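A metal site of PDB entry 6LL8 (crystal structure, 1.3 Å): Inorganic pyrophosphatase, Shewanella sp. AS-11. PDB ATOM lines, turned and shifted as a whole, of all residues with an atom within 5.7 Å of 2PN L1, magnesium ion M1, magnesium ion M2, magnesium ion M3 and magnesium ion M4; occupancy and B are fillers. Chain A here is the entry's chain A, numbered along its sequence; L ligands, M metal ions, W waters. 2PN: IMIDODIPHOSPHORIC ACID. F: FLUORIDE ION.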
ATOM      1  N   HIS A   9     -21.715  -6.189  23.953  1.00  0.00           N
ATOM      2  CA  HIS A   9     -22.363  -6.805  22.796  1.00  0.00           C
ATOM      3  C   HIS A   9     -22.964  -8.163  23.116  1.00  0.00           C
ATOM      4  O   HIS A   9     -22.489  -8.893  23.991  1.00  0.00           O
ATOM      5  CB  HIS A   9     -21.448  -6.854  21.562  1.00  0.00           C
ATOM      6  CG  HIS A   9     -20.077  -7.432  21.725  1.00  0.00           C
ATOM      7  ND1 HIS A   9     -19.826  -8.794  21.826  1.00  0.00           N
ATOM      8  CD2 HIS A   9     -18.860  -6.829  21.725  1.00  0.00           C
ATOM      9  CE1 HIS A   9     -18.480  -8.945  21.917  1.00  0.00           C
ATOM     10  NE2 HIS A   9     -17.868  -7.758  21.861  1.00  0.00           N
ATOM     11  N   ASP A  13     -17.583 -10.798  24.928  1.00  0.00           N
ATOM     12  CA  ASP A  13     -16.194 -11.165  25.173  1.00  0.00           C
ATOM     13  C   ASP A  13     -15.693 -10.485  26.447  1.00  0.00           C
ATOM     14  O   ASP A  13     -16.457  -9.810  27.157  1.00  0.00           O
ATOM     15  CB  ASP A  13     -15.364 -10.860  23.957  1.00  0.00           C
ATOM     16  CG  ASP A  13     -15.471  -9.415  23.485  1.00  0.00           C
ATOM     17  OD1 ASP A  13     -15.970  -8.533  24.230  1.00  0.00           O
ATOM     18  OD2 ASP A  13     -15.038  -9.113  22.339  1.00  0.00           O
ATOM     19  N   SER A  14     -14.432 -10.659  26.745  1.00  0.00           N
ATOM     20  CA  SER A  14     -13.866 -10.124  27.986  1.00  0.00           C
ATOM     21  C   SER A  14     -14.011  -8.604  28.030  1.00  0.00           C
ATOM     22  O   SER A  14     -14.269  -8.068  29.121  1.00  0.00           O
ATOM     23  CB  SER A  14     -12.452 -10.589  28.188  1.00  0.00           C
ATOM     24  OG  SER A  14     -12.407 -11.984  28.299  1.00  0.00           O
ATOM     25  N   ASP A  15     -13.763  -7.905  26.953  1.00  0.00           N
ATOM     26  CA  ASP A  15     -13.913  -6.447  26.983  1.00  0.00           C
ATOM     27  C   ASP A  15     -15.331  -6.064  27.351  1.00  0.00           C
ATOM     28  O   ASP A  15     -15.545  -5.178  28.196  1.00  0.00           O
ATOM     29  CB  ASP A  15     -13.513  -5.888  25.622  1.00  0.00           C
ATOM     30  CG  ASP A  15     -13.294  -4.408  25.493  1.00  0.00           C
ATOM     31  OD1 ASP A  15     -13.010  -3.762  26.549  1.00  0.00           O
ATOM     32  OD2 ASP A  15     -13.326  -3.882  24.360  1.00  0.00           O
ATOM     33  N   SER A  16     -16.319  -6.694  26.758  1.00  0.00           N
ATOM     34  CA  SER A  16     -17.724  -6.397  27.043  1.00  0.00           C
ATOM     35  C   SER A  16     -18.081  -6.721  28.494  1.00  0.00           C
ATOM     36  O   SER A  16     -18.893  -6.008  29.078  1.00  0.00           O
ATOM     37  CB  SER A  16     -18.641  -7.129  26.078  1.00  0.00           C
ATOM     38  OG  SER A  16     -18.797  -6.458  24.840  1.00  0.00           O
ATOM     39  N   ASP A  73     -18.611  -1.369  23.920  1.00  0.00           N
ATOM     40  CA  ASP A  73     -17.855  -2.260  23.011  1.00  0.00           C
ATOM     41  C   ASP A  73     -18.608  -2.566  21.718  1.00  0.00           C
ATOM     42  O   ASP A  73     -18.226  -3.535  21.046  1.00  0.00           O
ATOM     43  CB  ASP A  73     -17.404  -3.510  23.744  1.00  0.00           C
ATOM     44  CG  ASP A  73     -16.402  -4.404  23.095  1.00  0.00           C
ATOM     45  OD1 ASP A  73     -15.396  -3.906  22.509  1.00  0.00           O
ATOM     46  OD2 ASP A  73     -16.590  -5.626  23.239  1.00  0.00           O
ATOM     47  N   ASP A  94     -16.655   2.817  23.460  1.00  0.00           N
ATOM     48  CA  ASP A  94     -16.358   1.833  22.401  1.00  0.00           C
ATOM     49  C   ASP A  94     -15.107   2.218  21.653  1.00  0.00           C
ATOM     50  O   ASP A  94     -14.537   3.301  21.831  1.00  0.00           O
ATOM     51  CB  ASP A  94     -17.561   1.716  21.451  1.00  0.00           C
ATOM     52  CG  ASP A  94     -17.497   0.559  20.480  1.00  0.00           C
ATOM     53  OD1 ASP A  94     -16.788  -0.444  20.809  1.00  0.00           O
ATOM     54  OD2 ASP A  94     -18.139   0.633  19.431  1.00  0.00           O
ATOM     55  N   HIS A  95     -14.722   1.340  20.741  1.00  0.00           N
ATOM     56  CA  HIS A  95     -13.533   1.460  19.866  1.00  0.00           C
ATOM     57  C   HIS A  95     -13.800   0.818  18.500  1.00  0.00           C
ATOM     58  O   HIS A  95     -12.859   0.421  17.821  1.00  0.00           O
ATOM     59  CB  HIS A  95     -12.305   0.882  20.559  1.00  0.00           C
ATOM     60  CG  HIS A  95     -12.334  -0.596  20.862  1.00  0.00           C
ATOM     61  ND1 HIS A  95     -11.218  -1.370  20.668  1.00  0.00           N
ATOM     62  CD2 HIS A  95     -13.276  -1.419  21.400  1.00  0.00           C
ATOM     63  CE1 HIS A  95     -11.511  -2.610  21.086  1.00  0.00           C
ATOM     64  NE2 HIS A  95     -12.742  -2.688  21.534  1.00  0.00           N
ATOM     65  N   HIS A  96     -15.059   0.717  18.103  1.00  0.00           N
ATOM     66  CA  HIS A  96     -15.478   0.212  16.785  1.00  0.00           C
ATOM     67  C   HIS A  96     -15.899   1.344  15.863  1.00  0.00           C
ATOM     68  O   HIS A  96     -16.072   2.494  16.306  1.00  0.00           O
ATOM     69  CB  HIS A  96     -16.636  -0.795  16.914  1.00  0.00           C
ATOM     70  CG  HIS A  96     -16.230  -2.095  17.531  1.00  0.00           C
ATOM     71  ND1 HIS A  96     -16.168  -2.301  18.910  1.00  0.00           N
ATOM     72  CD2 HIS A  96     -15.868  -3.279  16.962  1.00  0.00           C
ATOM     73  CE1 HIS A  96     -15.757  -3.545  19.124  1.00  0.00           C
ATOM     74  NE2 HIS A  96     -15.585  -4.173  17.958  1.00  0.00           N
ATOM     75  N   GLY A 115      -7.117   0.131  21.069  1.00  0.00           N
ATOM     76  CA  GLY A 115      -7.139  -1.336  21.106  1.00  0.00           C
ATOM     77  C   GLY A 115      -8.207  -1.977  21.939  1.00  0.00           C
ATOM     78  O   GLY A 115      -8.478  -3.139  21.705  1.00  0.00           O
ATOM     79  N   CYS A 116      -8.810  -1.273  22.887  1.00  0.00           N
ATOM     80  CA  CYS A 116      -9.738  -1.921  23.826  1.00  0.00           C
ATOM     81  C   CYS A 116     -10.714  -0.906  24.408  1.00  0.00           C
ATOM     82  O   CYS A 116     -10.276   0.197  24.775  1.00  0.00           O
ATOM     83  CB  CYS A 116      -8.939  -2.628  24.900  1.00  0.00           C
ATOM     84  SG  CYS A 116      -9.943  -3.577  26.052  1.00  0.00           S
ATOM     85  N   SER A 117     -11.978  -1.289  24.592  1.00  0.00           N
ATOM     86  CA  SER A 117     -12.910  -0.383  25.263  1.00  0.00           C
ATOM     87  C   SER A 117     -12.423  -0.048  26.659  1.00  0.00           C
ATOM     88  O   SER A 117     -12.656   1.068  27.155  1.00  0.00           O
ATOM     89  CB  SER A 117     -14.304  -0.981  25.368  1.00  0.00           C
ATOM     90  OG  SER A 117     -14.886  -1.262  24.125  1.00  0.00           O
ATOM     91  N   SER A 146      -6.274  -9.006  26.002  1.00  0.00           N
ATOM     92  CA  SER A 146      -7.053  -9.876  25.113  1.00  0.00           C
ATOM     93  C   SER A 146      -7.347  -9.144  23.804  1.00  0.00           C
ATOM     94  O   SER A 146      -7.040  -9.658  22.717  1.00  0.00           O
ATOM     95  CB  SER A 146      -8.317 -10.333  25.789  1.00  0.00           C
ATOM     96  OG  SER A 146      -8.930 -11.280  24.973  1.00  0.00           O
ATOM     97  N   ASP A 147      -7.956  -7.968  23.895  1.00  0.00           N
ATOM     98  CA  ASP A 147      -8.344  -7.239  22.674  1.00  0.00           C
ATOM     99  C   ASP A 147      -7.144  -6.871  21.822  1.00  0.00           C
ATOM    100  O   ASP A 147      -7.254  -6.875  20.593  1.00  0.00           O
ATOM    101  CB  ASP A 147      -9.101  -5.975  23.036  1.00  0.00           C
ATOM    102  CG  ASP A 147     -10.598  -6.139  22.999  1.00  0.00           C
ATOM    103  OD1 ASP A 147     -11.045  -7.244  23.285  1.00  0.00           O
ATOM    104  OD2 ASP A 147     -11.332  -5.136  22.802  1.00  0.00           O
ATOM    105  N   ASP A 202     -17.300 -16.447  19.399  1.00  0.00           N
ATOM    106  CA  ASP A 202     -16.862 -15.050  19.238  1.00  0.00           C
ATOM    107  C   ASP A 202     -17.418 -14.557  17.911  1.00  0.00           C
ATOM    108  O   ASP A 202     -16.648 -14.283  16.984  1.00  0.00           O
ATOM    109  CB  ASP A 202     -15.363 -14.957  19.329  1.00  0.00           C
ATOM    110  CG  ASP A 202     -14.748 -13.590  19.231  1.00  0.00           C
ATOM    111  OD1 ASP A 202     -15.518 -12.610  19.272  1.00  0.00           O
ATOM    112  OD2 ASP A 202     -13.486 -13.563  19.196  1.00  0.00           O
ATOM    113  N   LYS A 204     -20.262 -12.297  15.564  1.00  0.00           N
ATOM    114  CA  LYS A 204     -21.020 -11.055  15.450  1.00  0.00           C
ATOM    115  C   LYS A 204     -21.726 -11.009  14.104  1.00  0.00           C
ATOM    116  O   LYS A 204     -21.140 -11.368  13.087  1.00  0.00           O
ATOM    117  CB  LYS A 204     -20.101  -9.838  15.545  1.00  0.00           C
ATOM    118  CG  LYS A 204     -19.442  -9.698  16.913  1.00  0.00           C
ATOM    119  CD  LYS A 204     -18.464  -8.532  16.923  1.00  0.00           C
ATOM    120  CE  LYS A 204     -17.798  -8.369  18.286  1.00  0.00           C
ATOM    121  NZ  LYS A 204     -16.858  -7.235  18.261  1.00  0.00           N
ATOM    122  N   PHE A 206     -23.414  -8.411  11.322  1.00  0.00           N
ATOM    123  CA  PHE A 206     -23.263  -7.065  10.753  1.00  0.00           C
ATOM    124  C   PHE A 206     -24.330  -6.872   9.707  1.00  0.00           C
ATOM    125  O   PHE A 206     -24.518  -7.726   8.829  1.00  0.00           O
ATOM    126  CB  PHE A 206     -21.899  -6.911  10.100  1.00  0.00           C
ATOM    127  CG  PHE A 206     -20.764  -7.040  11.069  1.00  0.00           C
ATOM    128  CD1 PHE A 206     -20.234  -8.281  11.386  1.00  0.00           C
ATOM    129  CD2 PHE A 206     -20.269  -5.932  11.738  1.00  0.00           C
ATOM    130  CE1 PHE A 206     -19.241  -8.423  12.317  1.00  0.00           C
ATOM    131  CE2 PHE A 206     -19.244  -6.064  12.654  1.00  0.00           C
ATOM    132  CZ  PHE A 206     -18.736  -7.314  12.965  1.00  0.00           C
ATOM    133  N   GLN A 217     -14.809 -15.631  14.986  1.00  0.00           N
ATOM    134  CA  GLN A 217     -13.345 -15.660  15.109  1.00  0.00           C
ATOM    135  C   GLN A 217     -12.954 -16.626  16.207  1.00  0.00           C
ATOM    136  O   GLN A 217     -13.608 -16.666  17.252  1.00  0.00           O
ATOM    137  CB  GLN A 217     -12.790 -14.268  15.379  1.00  0.00           C
ATOM    138  CG  GLN A 217     -11.259 -14.252  15.436  1.00  0.00           C
ATOM    139  CD  GLN A 217     -10.651 -12.881  15.411  1.00  0.00           C
ATOM    140  OE1 GLN A 217     -11.223 -11.934  15.935  1.00  0.00           O
ATOM    141  NE2 GLN A 217      -9.497 -12.736  14.771  1.00  0.00           N
ATOM    142  N   GLU A 219      -9.344 -17.230  17.953  1.00  0.00           N
ATOM    143  CA  GLU A 219      -7.926 -16.923  18.159  1.00  0.00           C
ATOM    144  C   GLU A 219      -7.288 -18.020  18.992  1.00  0.00           C
ATOM    145  O   GLU A 219      -7.785 -18.376  20.066  1.00  0.00           O
ATOM    146  CB  GLU A 219      -7.767 -15.608  18.933  1.00  0.00           C
ATOM    147  CG  GLU A 219      -8.286 -14.355  18.251  1.00  0.00           C
ATOM    148  CD  GLU A 219      -8.580 -13.286  19.285  1.00  0.00           C
ATOM    149  OE1 GLU A 219      -9.380 -13.581  20.220  1.00  0.00           O
ATOM    150  OE2 GLU A 219      -7.988 -12.225  19.222  1.00  0.00           O
ATOM    151  N   SER A 293      -7.148  -8.658  13.375  1.00  0.00           N
ATOM    152  CA  SER A 293      -8.230  -7.800  13.869  1.00  0.00           C
ATOM    153  C   SER A 293      -9.464  -7.842  12.968  1.00  0.00           C
ATOM    154  O   SER A 293      -9.387  -7.425  11.788  1.00  0.00           O
ATOM    155  CB  SER A 293      -7.751  -6.402  13.954  1.00  0.00           C
ATOM    156  OG  SER A 293      -8.827  -5.514  14.230  1.00  0.00           O
ATOM    157  N   ARG A 294     -10.597  -8.242  13.509  1.00  0.00           N
ATOM    158  CA  ARG A 294     -11.851  -8.175  12.752  1.00  0.00           C
ATOM    159  C   ARG A 294     -12.235  -6.715  12.512  1.00  0.00           C
ATOM    160  O   ARG A 294     -12.521  -6.330  11.366  1.00  0.00           O
ATOM    161  CB  ARG A 294     -12.915  -8.998  13.483  1.00  0.00           C
ATOM    162  CG  ARG A 294     -14.304  -8.945  12.853  1.00  0.00           C
ATOM    163  CD  ARG A 294     -15.278  -9.951  13.443  1.00  0.00           C
ATOM    164  NE  ARG A 294     -15.308  -9.865  14.883  1.00  0.00           N
ATOM    165  CZ  ARG A 294     -15.567 -10.853  15.724  1.00  0.00           C
ATOM    166  NH1 ARG A 294     -16.121 -11.981  15.308  1.00  0.00           N
ATOM    167  NH2 ARG A 294     -15.289 -10.706  17.003  1.00  0.00           N
ATOM    168  N   LYS A 295     -12.233  -5.877  13.543  1.00  0.00           N
ATOM    169  CA  LYS A 295     -12.708  -4.489  13.375  1.00  0.00           C
ATOM    170  C   LYS A 295     -11.828  -3.701  12.388  1.00  0.00           C
ATOM    171  O   LYS A 295     -12.350  -2.819  11.723  1.00  0.00           O
ATOM    172  CB  LYS A 295     -12.813  -3.718  14.696  1.00  0.00           C
ATOM    173  CG  LYS A 295     -11.489  -3.347  15.328  1.00  0.00           C
ATOM    174  CD  LYS A 295     -11.612  -2.421  16.555  1.00  0.00           C
ATOM    175  CE  LYS A 295     -12.398  -2.994  17.704  1.00  0.00           C
ATOM    176  NZ  LYS A 295     -11.807  -4.251  18.235  1.00  0.00           N
ATOM    177  N   LYS A 296     -10.521  -3.992  12.314  1.00  0.00           N
ATOM    178  CA  LYS A 296      -9.624  -3.129  11.535  1.00  0.00           C
ATOM    179  C   LYS A 296      -9.272  -3.743  10.195  1.00  0.00           C
ATOM    180  O   LYS A 296      -9.091  -3.005   9.216  1.00  0.00           O
ATOM    181  CB  LYS A 296      -8.367  -2.799  12.342  1.00  0.00           C
ATOM    182  CG  LYS A 296      -7.436  -1.791  11.742  1.00  0.00           C
ATOM    183  CD  LYS A 296      -6.330  -1.404  12.686  1.00  0.00           C
ATOM    184  CE  LYS A 296      -5.265  -0.518  12.071  1.00  0.00           C
ATOM    185  NZ  LYS A 296      -5.808   0.768  11.640  1.00  0.00           N
HETATM  186  P1  2PN L   1     -13.822  -6.613  19.929  1.00  0.00           P
HETATM  187  O1  2PN L   1     -15.259  -6.810  20.427  1.00  0.00           O
HETATM  188  O2  2PN L   1     -12.948  -7.804  20.231  1.00  0.00           O
HETATM  189  O3  2PN L   1     -13.243  -5.319  20.463  1.00  0.00           O
HETATM  190  N1  2PN L   1     -13.915  -6.456  18.296  1.00  0.00           N
HETATM  191  P2  2PN L   1     -13.460  -7.376  17.006  1.00  0.00           P
HETATM  192  O4  2PN L   1     -14.719  -7.455  16.146  1.00  0.00           O
HETATM  193  O5  2PN L   1     -13.070  -8.745  17.522  1.00  0.00           O
HETATM  194  O6  2PN L   1     -12.333  -6.669  16.298  1.00  0.00           O
HETATM  195  F     F L   2     -13.972  -6.529  22.822  1.00  0.00           F
HETATM  196 MG    MG M   1     -13.382  -4.659  22.396  1.00  0.00          MG
HETATM  197 MG    MG M   2     -15.771  -7.178  22.289  1.00  0.00          MG
HETATM  198 MG    MG M   3     -12.498  -9.517  19.328  1.00  0.00          MG
HETATM  199 MG    MG M   4     -12.736  -8.344  22.426  1.00  0.00          MG
HETATM  200  O   HOH W   1     -14.379 -10.241  19.913  1.00  0.00           O
HETATM  201  O   HOH W   2     -10.337  -6.396  19.958  1.00  0.00           O
HETATM  202  O   HOH W   3      -9.705  -6.121  16.659  1.00  0.00           O
HETATM  203  O   HOH W   4     -10.633  -9.309  16.128  1.00  0.00           O
HETATM  204  O   HOH W   5     -12.173 -11.388  18.504  1.00  0.00           O
HETATM  205  O   HOH W   6     -15.981  -5.826  14.450  1.00  0.00           O
HETATM  206  O   HOH W   7     -12.308  -9.180  24.647  1.00  0.00           O
HETATM  207  O   HOH W   8     -10.462  -9.009  18.965  1.00  0.00           O
HETATM  208  O   HOH W   9     -11.770 -10.177  21.253  1.00  0.00           O
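NZ of Lys 204 is in salt-bridge range of O4 of 2PN L1 (3.0 Å).
NE of Arg 294 lies within salt-bridge range of O4 of 2PN L1 (2.8 Å).
A nitrogen (N1) of 2PN L1 sits at hydrogen-bond distance from a ring nitrogen (NE2) of His 96, at 2.8 Å.
The backbone NH (N) of Lys 295 is in hydrogen-bond range of an oxygen (O6) of 2PN L1 (2.9 Å).
An oxygen (O6) of 2PN L1 lies within salt-bridge range of the side-chain amino group (NZ) of Lys 295 (3.1 Å).
O of Asp 73 sits close to ND1 of His 96.
OD1 of Asp 73 lies close to OG of Ser 117 (3.1 Å).
The backbone NH (N) of Ser 16 lies close to the side-chain carboxylate (OD1) of Asp 13.
The backbone NH of Ser 117 lies close to the side-chain carboxylate of Asp 15.
The backbone NH of His 9 sits at hydrogen-bond distance from the side-chain hydroxyl of Ser 16, 3.1 Å away.
A ring nitrogen (ND1) of His 95 sits close to the backbone carbonyl oxygen of Gly 115 (3.4 Å).
OD1 of Asp 94 lies within hydrogen-bond range of ND1 of His 96 (2.7 Å).
The side-chain hydroxyl (OG) of Ser 293 sits close to the backbone NH (N) of Lys 295 (3.5 Å).
Hydrophobic or aromatic side chains that line 2PN L1: His 9, His 95 and His 96.
Of the 23 residues printed, 9 come within 4 Å of 2PN L1.
The nearest printed residue that does not touch magnesium ion M1 is Ser 117 (4.1 Å).
Along chain A the residues within 4 Å of magnesium ion M2 span positions 9 to 73.
The nearest printed residue that does not touch magnesium ion M2 is Ser 16 (4.02 Å).
Residues that only touch magnesium ion M3: Arg 294.
Within 4 Å of magnesium ion M3: Asp 13 and Arg 294.
The nearest printed residue that does not touch magnesium ion M3 is Asp 202 (4.2 Å).
Magnesium ion M1 is bound by F of F L2 (2.0 Å), O3 of 2PN L1 (2.0 Å), OD2 of Asp 15 (2.1 Å), OD2 of Asp 147 (2.1 Å), OD1 of Asp 73 (2.2 Å) and NE2 of His 95 (2.2 Å).
Magnesium ion M1 has six donor atoms within binding distance.
Magnesium ion M2 is bound by an oxygen (O1) of 2PN L1.
Magnesium ion M2 is bound by F of F L2 (2.0 Å).
Magnesium ion M2 is bound by the side-chain carboxylate (OD2) of Asp 73 (2.0 Å).
Magnesium ion M2 is bound by the side-chain carboxylate (OD2) of Asp 13 (2.1 Å).
Magnesium ion M2 is bound by NE2 of His 9 (2.2 Å).
Magnesium ion M2 is bound by the side-chain carboxylate (OD1) of Asp 13 (2.4 Å).
Magnesium ion M3 is bound by an oxygen (O2) of 2PN L1 (2.0 Å), an oxygen (O5) of 2PN L1 (2.0 Å), water W5 (2.1 Å), water W1 (2.1 Å), water W8 (2.1 Å) and water W9 (2.2 Å).
Magnesium ion M3 has six donor atoms within binding distance.
Magnesium ion M4 is bound by the side-chain carboxylate (OD1) of Asp 147 (2.2 Å), a fluorine (F) of F L2 (2.2 Å), an oxygen (O2) of 2PN L1 (2.3 Å), water W9 (2.4 Å), water W7 (2.4 Å) and the side-chain carboxylate (OD2) of Asp 13 (2.4 Å).
Water W1 bridges the side-chain carboxylate (OD1) of Asp 202 (2.7 Å) and the guanidinium group (NH2) of Arg 294 (3.1 Å).
Water W5 bridges OD2 of Asp 202 (2.6 Å) and OE1 of Gln 217 (2.8 Å).
Water W3 lies within hydrogen-bond range of OG of Ser 293, O6 of 2PN L1 and NZ of Lys 295.
Water W4 lies within hydrogen-bond range of the side-chain amide oxygen (OE1) of Gln 217 (2.7 Å), the backbone NH (N) of Arg 294 (2.8 Å) and an oxygen (O6) of 2PN L1 (3.1 Å).
Water W2 lies within hydrogen-bond range of the side-chain amino group (NZ) of Lys 295 (3.1 Å) and the backbone carbonyl oxygen (O) of Asp 147 (3.2 Å).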
